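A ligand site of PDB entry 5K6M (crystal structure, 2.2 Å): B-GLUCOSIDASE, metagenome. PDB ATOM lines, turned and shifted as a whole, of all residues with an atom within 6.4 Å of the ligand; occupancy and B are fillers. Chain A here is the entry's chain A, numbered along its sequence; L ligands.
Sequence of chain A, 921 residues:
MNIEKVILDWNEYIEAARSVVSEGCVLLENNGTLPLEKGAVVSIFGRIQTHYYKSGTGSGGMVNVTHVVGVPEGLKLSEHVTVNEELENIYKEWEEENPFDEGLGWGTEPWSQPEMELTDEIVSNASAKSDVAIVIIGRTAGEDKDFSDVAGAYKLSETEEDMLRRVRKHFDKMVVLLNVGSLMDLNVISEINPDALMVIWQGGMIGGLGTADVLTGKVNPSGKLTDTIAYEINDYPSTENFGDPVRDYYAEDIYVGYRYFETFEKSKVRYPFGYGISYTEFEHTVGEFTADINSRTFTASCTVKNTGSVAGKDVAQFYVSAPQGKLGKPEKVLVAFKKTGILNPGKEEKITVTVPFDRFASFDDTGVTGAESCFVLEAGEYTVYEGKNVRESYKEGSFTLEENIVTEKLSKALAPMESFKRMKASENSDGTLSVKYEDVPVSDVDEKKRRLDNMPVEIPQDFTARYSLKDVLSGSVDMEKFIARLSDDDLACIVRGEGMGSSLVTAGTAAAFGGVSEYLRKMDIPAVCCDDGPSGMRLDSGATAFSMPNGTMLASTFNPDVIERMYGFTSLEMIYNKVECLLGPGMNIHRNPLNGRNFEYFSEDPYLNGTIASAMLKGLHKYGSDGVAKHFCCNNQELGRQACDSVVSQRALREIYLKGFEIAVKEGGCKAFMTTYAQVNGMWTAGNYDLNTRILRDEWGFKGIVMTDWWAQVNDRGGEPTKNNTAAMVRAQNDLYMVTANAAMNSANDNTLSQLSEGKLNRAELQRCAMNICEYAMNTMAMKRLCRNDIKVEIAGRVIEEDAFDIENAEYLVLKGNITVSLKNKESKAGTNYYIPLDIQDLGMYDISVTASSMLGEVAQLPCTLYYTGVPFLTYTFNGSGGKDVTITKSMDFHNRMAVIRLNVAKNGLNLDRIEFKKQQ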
ATOM      1  N   SER A  59     -20.617 -21.993  15.958  1.00  0.00           N
ATOM      2  CA  SER A  59     -20.378 -23.088  16.916  1.00  0.00           C
ATOM      3  C   SER A  59     -19.816 -22.658  18.283  1.00  0.00           C
ATOM      4  O   SER A  59     -20.197 -23.217  19.317  1.00  0.00           O
ATOM      5  CB  SER A  59     -19.421 -24.117  16.309  1.00  0.00           C
ATOM      6  OG  SER A  59     -18.146 -23.525  16.044  1.00  0.00           O
ATOM      7  N   GLY A  60     -18.921 -21.676  18.270  1.00  0.00           N
ATOM      8  CA  GLY A  60     -18.345 -21.102  19.487  1.00  0.00           C
ATOM      9  C   GLY A  60     -19.070 -19.884  20.036  1.00  0.00           C
ATOM     10  O   GLY A  60     -18.483 -19.097  20.782  1.00  0.00           O
ATOM     11  N   GLU A 143     -18.415 -17.871  12.064  1.00  0.00           N
ATOM     12  CA  GLU A 143     -18.215 -19.022  11.213  1.00  0.00           C
ATOM     13  C   GLU A 143     -18.858 -18.782   9.839  1.00  0.00           C
ATOM     14  O   GLU A 143     -19.937 -18.212   9.741  1.00  0.00           O
ATOM     15  CB  GLU A 143     -18.809 -20.230  11.917  1.00  0.00           C
ATOM     16  CG  GLU A 143     -18.100 -21.536  11.649  1.00  0.00           C
ATOM     17  CD  GLU A 143     -18.648 -22.669  12.493  1.00  0.00           C
ATOM     18  OE1 GLU A 143     -18.877 -22.459  13.714  1.00  0.00           O
ATOM     19  OE2 GLU A 143     -18.853 -23.760  11.934  1.00  0.00           O
ATOM     20  N   ASP A 144     -18.155 -19.191   8.777  1.00  0.00           N
ATOM     21  CA  ASP A 144     -18.651 -19.145   7.374  1.00  0.00           C
ATOM     22  C   ASP A 144     -18.875 -17.775   6.706  1.00  0.00           C
ATOM     23  O   ASP A 144     -19.179 -17.735   5.502  1.00  0.00           O
ATOM     24  CB  ASP A 144     -19.909 -20.035   7.193  1.00  0.00           C
ATOM     25  CG  ASP A 144     -19.555 -21.492   7.010  1.00  0.00           C
ATOM     26  OD1 ASP A 144     -18.858 -21.816   6.024  1.00  0.00           O
ATOM     27  OD2 ASP A 144     -19.964 -22.315   7.854  1.00  0.00           O
ATOM     28  N   MET A 500     -24.896 -35.053  15.279  1.00  0.00           N
ATOM     29  CA  MET A 500     -25.033 -34.343  16.561  1.00  0.00           C
ATOM     30  C   MET A 500     -26.244 -34.851  17.340  1.00  0.00           C
ATOM     31  O   MET A 500     -27.173 -35.439  16.766  1.00  0.00           O
ATOM     32  CB  MET A 500     -25.177 -32.832  16.329  1.00  0.00           C
ATOM     33  CG  MET A 500     -23.919 -32.194  15.759  1.00  0.00           C
ATOM     34  SD  MET A 500     -24.017 -30.398  15.643  1.00  0.00           S
ATOM     35  CE  MET A 500     -23.926 -29.909  17.364  1.00  0.00           C
ATOM     36  N   ALA A 510     -22.115 -32.219  20.662  1.00  0.00           N
ATOM     37  CA  ALA A 510     -21.640 -32.326  19.291  1.00  0.00           C
ATOM     38  C   ALA A 510     -21.461 -33.756  18.835  1.00  0.00           C
ATOM     39  O   ALA A 510     -21.740 -34.064  17.683  1.00  0.00           O
ATOM     40  CB  ALA A 510     -20.332 -31.560  19.125  1.00  0.00           C
ATOM     41  N   ASP A 532     -18.933 -28.308  21.686  1.00  0.00           N
ATOM     42  CA  ASP A 532     -18.479 -26.926  21.581  1.00  0.00           C
ATOM     43  C   ASP A 532     -18.709 -26.231  22.937  1.00  0.00           C
ATOM     44  O   ASP A 532     -19.569 -26.651  23.704  1.00  0.00           O
ATOM     45  CB  ASP A 532     -19.263 -26.158  20.523  1.00  0.00           C
ATOM     46  CG  ASP A 532     -19.021 -26.658  19.134  1.00  0.00           C
ATOM     47  OD1 ASP A 532     -17.837 -26.741  18.724  1.00  0.00           O
ATOM     48  OD2 ASP A 532     -20.017 -26.955  18.445  1.00  0.00           O
ATOM     49  N   ARG A 538     -21.934 -25.420  24.620  1.00  0.00           N
ATOM     50  CA  ARG A 538     -23.081 -25.159  23.761  1.00  0.00           C
ATOM     51  C   ARG A 538     -24.003 -26.362  23.890  1.00  0.00           C
ATOM     52  O   ARG A 538     -23.655 -27.460  23.472  1.00  0.00           O
ATOM     53  CB  ARG A 538     -22.603 -25.016  22.317  1.00  0.00           C
ATOM     54  CG  ARG A 538     -23.679 -25.115  21.253  1.00  0.00           C
ATOM     55  CD  ARG A 538     -23.069 -25.352  19.899  1.00  0.00           C
ATOM     56  NE  ARG A 538     -24.089 -25.651  18.907  1.00  0.00           N
ATOM     57  CZ  ARG A 538     -23.833 -25.940  17.628  1.00  0.00           C
ATOM     58  NH1 ARG A 538     -22.584 -25.980  17.166  1.00  0.00           N
ATOM     59  NH2 ARG A 538     -24.850 -26.211  16.820  1.00  0.00           N
ATOM     60  N   LEU A 583     -14.595 -28.606  22.582  1.00  0.00           N
ATOM     61  CA  LEU A 583     -14.004 -28.414  21.247  1.00  0.00           C
ATOM     62  C   LEU A 583     -13.341 -27.036  21.132  1.00  0.00           C
ATOM     63  O   LEU A 583     -13.806 -26.140  20.443  1.00  0.00           O
ATOM     64  CB  LEU A 583     -15.058 -28.632  20.154  1.00  0.00           C
ATOM     65  CG  LEU A 583     -15.706 -30.031  20.163  1.00  0.00           C
ATOM     66  CD1 LEU A 583     -16.841 -30.088  19.146  1.00  0.00           C
ATOM     67  CD2 LEU A 583     -14.684 -31.120  19.887  1.00  0.00           C
ATOM     68  N   ARG A 597     -13.597 -15.766  12.021  1.00  0.00           N
ATOM     69  CA  ARG A 597     -13.431 -16.541  13.256  1.00  0.00           C
ATOM     70  C   ARG A 597     -12.312 -16.038  14.174  1.00  0.00           C
ATOM     71  O   ARG A 597     -12.031 -16.684  15.180  1.00  0.00           O
ATOM     72  CB  ARG A 597     -13.237 -18.036  12.947  1.00  0.00           C
ATOM     73  CG  ARG A 597     -14.528 -18.720  12.544  1.00  0.00           C
ATOM     74  CD  ARG A 597     -14.414 -20.232  12.509  1.00  0.00           C
ATOM     75  NE  ARG A 597     -14.830 -20.873  13.763  1.00  0.00           N
ATOM     76  CZ  ARG A 597     -15.114 -22.175  13.898  1.00  0.00           C
ATOM     77  NH1 ARG A 597     -15.004 -23.017  12.867  1.00  0.00           N
ATOM     78  NH2 ARG A 597     -15.503 -22.652  15.077  1.00  0.00           N
ATOM     79  N   GLU A 600     -12.512 -16.171  18.211  1.00  0.00           N
ATOM     80  CA  GLU A 600     -12.258 -17.365  19.037  1.00  0.00           C
ATOM     81  C   GLU A 600     -10.858 -17.951  18.874  1.00  0.00           C
ATOM     82  O   GLU A 600     -10.572 -19.007  19.417  1.00  0.00           O
ATOM     83  CB  GLU A 600     -13.352 -18.431  18.842  1.00  0.00           C
ATOM     84  CG  GLU A 600     -13.414 -19.127  17.493  1.00  0.00           C
ATOM     85  CD  GLU A 600     -14.650 -20.007  17.345  1.00  0.00           C
ATOM     86  OE1 GLU A 600     -15.030 -20.700  18.325  1.00  0.00           O
ATOM     87  OE2 GLU A 600     -15.253 -20.015  16.251  1.00  0.00           O
ATOM     88  N   LYS A 630      -8.094 -27.023  17.670  1.00  0.00           N
ATOM     89  CA  LYS A 630      -8.622 -26.885  16.320  1.00  0.00           C
ATOM     90  C   LYS A 630      -8.210 -25.552  15.712  1.00  0.00           C
ATOM     91  O   LYS A 630      -7.840 -24.637  16.450  1.00  0.00           O
ATOM     92  CB  LYS A 630     -10.143 -27.010  16.349  1.00  0.00           C
ATOM     93  CG  LYS A 630     -10.877 -25.863  17.003  1.00  0.00           C
ATOM     94  CD  LYS A 630     -12.342 -26.193  17.284  1.00  0.00           C
ATOM     95  CE  LYS A 630     -13.145 -24.940  17.608  1.00  0.00           C
ATOM     96  NZ  LYS A 630     -14.563 -25.234  17.928  1.00  0.00           N
ATOM     97  N   HIS A 631      -8.260 -25.388  14.389  1.00  0.00           N
ATOM     98  CA  HIS A 631      -8.501 -26.416  13.380  1.00  0.00           C
ATOM     99  C   HIS A 631      -7.146 -26.671  12.740  1.00  0.00           C
ATOM    100  O   HIS A 631      -6.515 -25.741  12.199  1.00  0.00           O
ATOM    101  CB  HIS A 631      -9.508 -25.914  12.352  1.00  0.00           C
ATOM    102  CG  HIS A 631     -10.741 -25.330  12.973  1.00  0.00           C
ATOM    103  ND1 HIS A 631     -10.852 -24.002  13.305  1.00  0.00           N
ATOM    104  CD2 HIS A 631     -11.912 -25.917  13.339  1.00  0.00           C
ATOM    105  CE1 HIS A 631     -12.039 -23.784  13.850  1.00  0.00           C
ATOM    106  NE2 HIS A 631     -12.698 -24.926  13.873  1.00  0.00           N
ATOM    107  N   ASN A 635      -6.691 -23.094   8.763  1.00  0.00           N
ATOM    108  CA  ASN A 635      -8.042 -22.599   8.560  1.00  0.00           C
ATOM    109  C   ASN A 635      -8.028 -21.117   9.004  1.00  0.00           C
ATOM    110  O   ASN A 635      -8.477 -20.776  10.105  1.00  0.00           O
ATOM    111  CB  ASN A 635      -9.003 -23.483   9.367  1.00  0.00           C
ATOM    112  CG  ASN A 635     -10.456 -23.093   9.208  1.00  0.00           C
ATOM    113  OD1 ASN A 635     -11.258 -23.384  10.081  1.00  0.00           O
ATOM    114  ND2 ASN A 635     -10.805 -22.431   8.102  1.00  0.00           N
ATOM    115  N   GLU A 638     -12.686 -18.035   6.361  1.00  0.00           N
ATOM    116  CA  GLU A 638     -13.989 -18.710   6.342  1.00  0.00           C
ATOM    117  C   GLU A 638     -14.558 -18.909   4.952  1.00  0.00           C
ATOM    118  O   GLU A 638     -15.178 -19.934   4.692  1.00  0.00           O
ATOM    119  CB  GLU A 638     -15.017 -17.976   7.223  1.00  0.00           C
ATOM    120  CG  GLU A 638     -14.719 -18.068   8.711  1.00  0.00           C
ATOM    121  CD  GLU A 638     -14.538 -19.506   9.186  1.00  0.00           C
ATOM    122  OE1 GLU A 638     -15.546 -20.248   9.287  1.00  0.00           O
ATOM    123  OE2 GLU A 638     -13.382 -19.886   9.437  1.00  0.00           O
ATOM    124  N   ARG A 641     -14.382 -22.279   2.766  1.00  0.00           N
ATOM    125  CA  ARG A 641     -13.619 -23.183   3.661  1.00  0.00           C
ATOM    126  C   ARG A 641     -13.850 -24.693   3.453  1.00  0.00           C
ATOM    127  O   ARG A 641     -13.093 -25.491   4.001  1.00  0.00           O
ATOM    128  CB  ARG A 641     -13.831 -22.822   5.145  1.00  0.00           C
ATOM    129  CG  ARG A 641     -15.257 -23.045   5.673  1.00  0.00           C
ATOM    130  CD  ARG A 641     -15.310 -22.965   7.186  1.00  0.00           C
ATOM    131  NE  ARG A 641     -16.652 -23.312   7.679  1.00  0.00           N
ATOM    132  CZ  ARG A 641     -16.950 -23.672   8.937  1.00  0.00           C
ATOM    133  NH1 ARG A 641     -16.024 -23.753   9.883  1.00  0.00           N
ATOM    134  NH2 ARG A 641     -18.211 -23.976   9.235  1.00  0.00           N
ATOM    135  N   MET A 674      -8.483 -31.457  16.171  1.00  0.00           N
ATOM    136  CA  MET A 674      -9.508 -31.472  15.124  1.00  0.00           C
ATOM    137  C   MET A 674      -8.879 -30.918  13.864  1.00  0.00           C
ATOM    138  O   MET A 674      -8.247 -29.870  13.916  1.00  0.00           O
ATOM    139  CB  MET A 674     -10.713 -30.611  15.507  1.00  0.00           C
ATOM    140  CG  MET A 674     -11.891 -30.711  14.549  1.00  0.00           C
ATOM    141  SD  MET A 674     -13.200 -29.487  14.861  1.00  0.00           S
ATOM    142  CE  MET A 674     -13.699 -30.019  16.498  1.00  0.00           C
ATOM    143  N   TYR A 677     -12.024 -28.206   7.473  1.00  0.00           N
ATOM    144  CA  TYR A 677     -12.873 -28.409   6.290  1.00  0.00           C
ATOM    145  C   TYR A 677     -12.126 -28.284   4.951  1.00  0.00           C
ATOM    146  O   TYR A 677     -12.679 -28.652   3.920  1.00  0.00           O
ATOM    147  CB  TYR A 677     -14.023 -27.382   6.284  1.00  0.00           C
ATOM    148  CG  TYR A 677     -15.144 -27.693   7.251  1.00  0.00           C
ATOM    149  CD1 TYR A 677     -15.837 -28.902   7.170  1.00  0.00           C
ATOM    150  CD2 TYR A 677     -15.535 -26.772   8.232  1.00  0.00           C
ATOM    151  CE1 TYR A 677     -16.870 -29.193   8.033  1.00  0.00           C
ATOM    152  CE2 TYR A 677     -16.575 -27.067   9.118  1.00  0.00           C
ATOM    153  CZ  TYR A 677     -17.240 -28.276   9.007  1.00  0.00           C
ATOM    154  OH  TYR A 677     -18.259 -28.578   9.872  1.00  0.00           O
ATOM    155  N   ASP A 709     -13.350 -32.236  11.292  1.00  0.00           N
ATOM    156  CA  ASP A 709     -14.366 -31.228  11.505  1.00  0.00           C
ATOM    157  C   ASP A 709     -15.716 -31.854  11.099  1.00  0.00           C
ATOM    158  O   ASP A 709     -15.739 -32.889  10.430  1.00  0.00           O
ATOM    159  CB  ASP A 709     -14.053 -29.959  10.696  1.00  0.00           C
ATOM    160  CG  ASP A 709     -14.530 -28.710  11.380  1.00  0.00           C
ATOM    161  OD1 ASP A 709     -15.545 -28.797  12.109  1.00  0.00           O
ATOM    162  OD2 ASP A 709     -13.894 -27.650  11.220  1.00  0.00           O
ATOM    163  N   TRP A 710     -16.815 -31.234  11.520  1.00  0.00           N
ATOM    164  CA  TRP A 710     -18.151 -31.857  11.432  1.00  0.00           C
ATOM    165  C   TRP A 710     -18.723 -31.949  10.016  1.00  0.00           C
ATOM    166  O   TRP A 710     -19.060 -30.925   9.402  1.00  0.00           O
ATOM    167  CB  TRP A 710     -19.144 -31.123  12.350  1.00  0.00           C
ATOM    168  CG  TRP A 710     -19.293 -31.782  13.687  1.00  0.00           C
ATOM    169  CD1 TRP A 710     -20.460 -32.193  14.264  1.00  0.00           C
ATOM    170  CD2 TRP A 710     -18.252 -32.118  14.617  1.00  0.00           C
ATOM    171  NE1 TRP A 710     -20.212 -32.748  15.493  1.00  0.00           N
ATOM    172  CE2 TRP A 710     -18.865 -32.710  15.740  1.00  0.00           C
ATOM    173  CE3 TRP A 710     -16.856 -31.946  14.618  1.00  0.00           C
ATOM    174  CZ2 TRP A 710     -18.139 -33.155  16.844  1.00  0.00           C
ATOM    175  CZ3 TRP A 710     -16.132 -32.383  15.727  1.00  0.00           C
ATOM    176  CH2 TRP A 710     -16.774 -32.992  16.827  1.00  0.00           C
ATOM    177  N   TRP A 711     -18.867 -33.183   9.532  1.00  0.00           N
ATOM    178  CA  TRP A 711     -19.264 -33.504   8.141  1.00  0.00           C
ATOM    179  C   TRP A 711     -18.236 -32.996   7.135  1.00  0.00           C
ATOM    180  O   TRP A 711     -18.594 -32.555   6.026  1.00  0.00           O
ATOM    181  CB  TRP A 711     -20.684 -33.003   7.812  1.00  0.00           C
ATOM    182  CG  TRP A 711     -21.709 -33.449   8.813  1.00  0.00           C
ATOM    183  CD1 TRP A 711     -22.226 -34.712   8.947  1.00  0.00           C
ATOM    184  CD2 TRP A 711     -22.345 -32.647   9.822  1.00  0.00           C
ATOM    185  NE1 TRP A 711     -23.128 -34.742   9.983  1.00  0.00           N
ATOM    186  CE2 TRP A 711     -23.224 -33.486  10.539  1.00  0.00           C
ATOM    187  CE3 TRP A 711     -22.251 -31.285  10.198  1.00  0.00           C
ATOM    188  CZ2 TRP A 711     -24.016 -33.020  11.606  1.00  0.00           C
ATOM    189  CZ3 TRP A 711     -23.032 -30.825  11.260  1.00  0.00           C
ATOM    190  CH2 TRP A 711     -23.905 -31.694  11.949  1.00  0.00           C
HETATM  191  C1  LIG L   1     -16.814 -26.050  13.290  1.00  0.00           C
HETATM  192  C2  LIG L   1     -16.052 -26.540  14.511  1.00  0.00           C
HETATM  193  C3  LIG L   1     -17.002 -27.120  15.555  1.00  0.00           C
HETATM  194  C4  LIG L   1     -17.860 -28.226  14.916  1.00  0.00           C
HETATM  195  C5  LIG L   1     -18.869 -28.849  15.885  1.00  0.00           C
HETATM  196  C6  LIG L   1     -17.853 -27.067  12.774  1.00  0.00           C
HETATM  197  O1  LIG L   1     -18.791 -26.419  11.891  1.00  0.00           O
HETATM  198  O2  LIG L   1     -15.849 -25.727  12.277  1.00  0.00           O
HETATM  199  O3  LIG L   1     -15.284 -25.452  15.039  1.00  0.00           O
HETATM  200  O4  LIG L   1     -16.261 -27.609  16.680  1.00  0.00           O
HETATM  201  O5  LIG L   1     -18.613 -27.681  13.832  1.00  0.00           O
HETATM  202  O6  LIG L   1     -19.881 -27.884  16.201  1.00  0.00           O
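The side-chain carboxylate (OD1) of Asp 532 lies within salt-bridge range of the side-chain amino group (NZ) of Lys 630 (3.7 Å). The side-chain carboxylate (OD2) of Asp 532 lies within salt-bridge range of the guanidinium group (NH1) of Arg 538, at 3.0 Å. The side-chain carboxylate of Glu 143 is in salt-bridge range of the guanidinium group of Arg 597 (3.6 Å). OG of Ser 59 sits at hydrogen-bond distance from OE1 of Glu 143 (2.7 Å). The guanidinium group (NH1) of Arg 597 sits at hydrogen-bond distance from a ring nitrogen (NE2) of His 631. The guanidinium group (NH2) of Arg 597 lies within hydrogen-bond range of the side-chain hydroxyl (OG) of Ser 59. The backbone carbonyl oxygen of Trp 710 lies within hydrogen-bond range of the side-chain hydroxyl of Tyr 677, 2.5 Å away. The guanidinium group of Arg 641 lies within salt-bridge range of the side-chain carboxylate of Glu 638, at 3.6 Å.
The side-chain carboxylate (OD2) of Asp 532 sits at hydrogen-bond distance from an oxygen (O6) of the ligand, at 2.4 Å. An oxygen (O1) of the ligand is in hydrogen-bond range of the side-chain carboxylate (OE2) of Glu 143 (2.7 Å). O3 of the ligand sits at hydrogen-bond distance from NH2 of Arg 597. A ring nitrogen (NE2) of His 631 sits at hydrogen-bond distance from an oxygen (O3) of the ligand (2.9 Å). The side-chain carboxylate (OD2) of Asp 709 lies within hydrogen-bond range of an oxygen (O2) of the ligand (2.9 Å). NZ of Lys 630 is in hydrogen-bond range of O3 of the ligand, 3.0 Å away. The side-chain hydroxyl of Tyr 677 lies within hydrogen-bond range of an oxygen (O1) of the ligand, 3.0 Å away. O2 of the ligand sits at hydrogen-bond distance from NH1 of Arg 641 (3.1 Å). NH1 of Arg 538 sits at hydrogen-bond distance from O6 of the ligand (3.4 Å).
Ser 59 touches the ligand. Leu 583 touches the ligand (CD1 to O4, 3.5 Å). CE of Met 674 touches O4 of the ligand, 3.5 Å away. CD2 of Trp 710 touches C5 of the ligand, 3.6 Å away. Within 4 Å of the ligand: Ser 59, Glu 143, Asp 532, Arg 538, Leu 583, Arg 597, Lys 630, His 631, Arg 641, Met 674, Tyr 677, Asp 709 and Trp 710.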
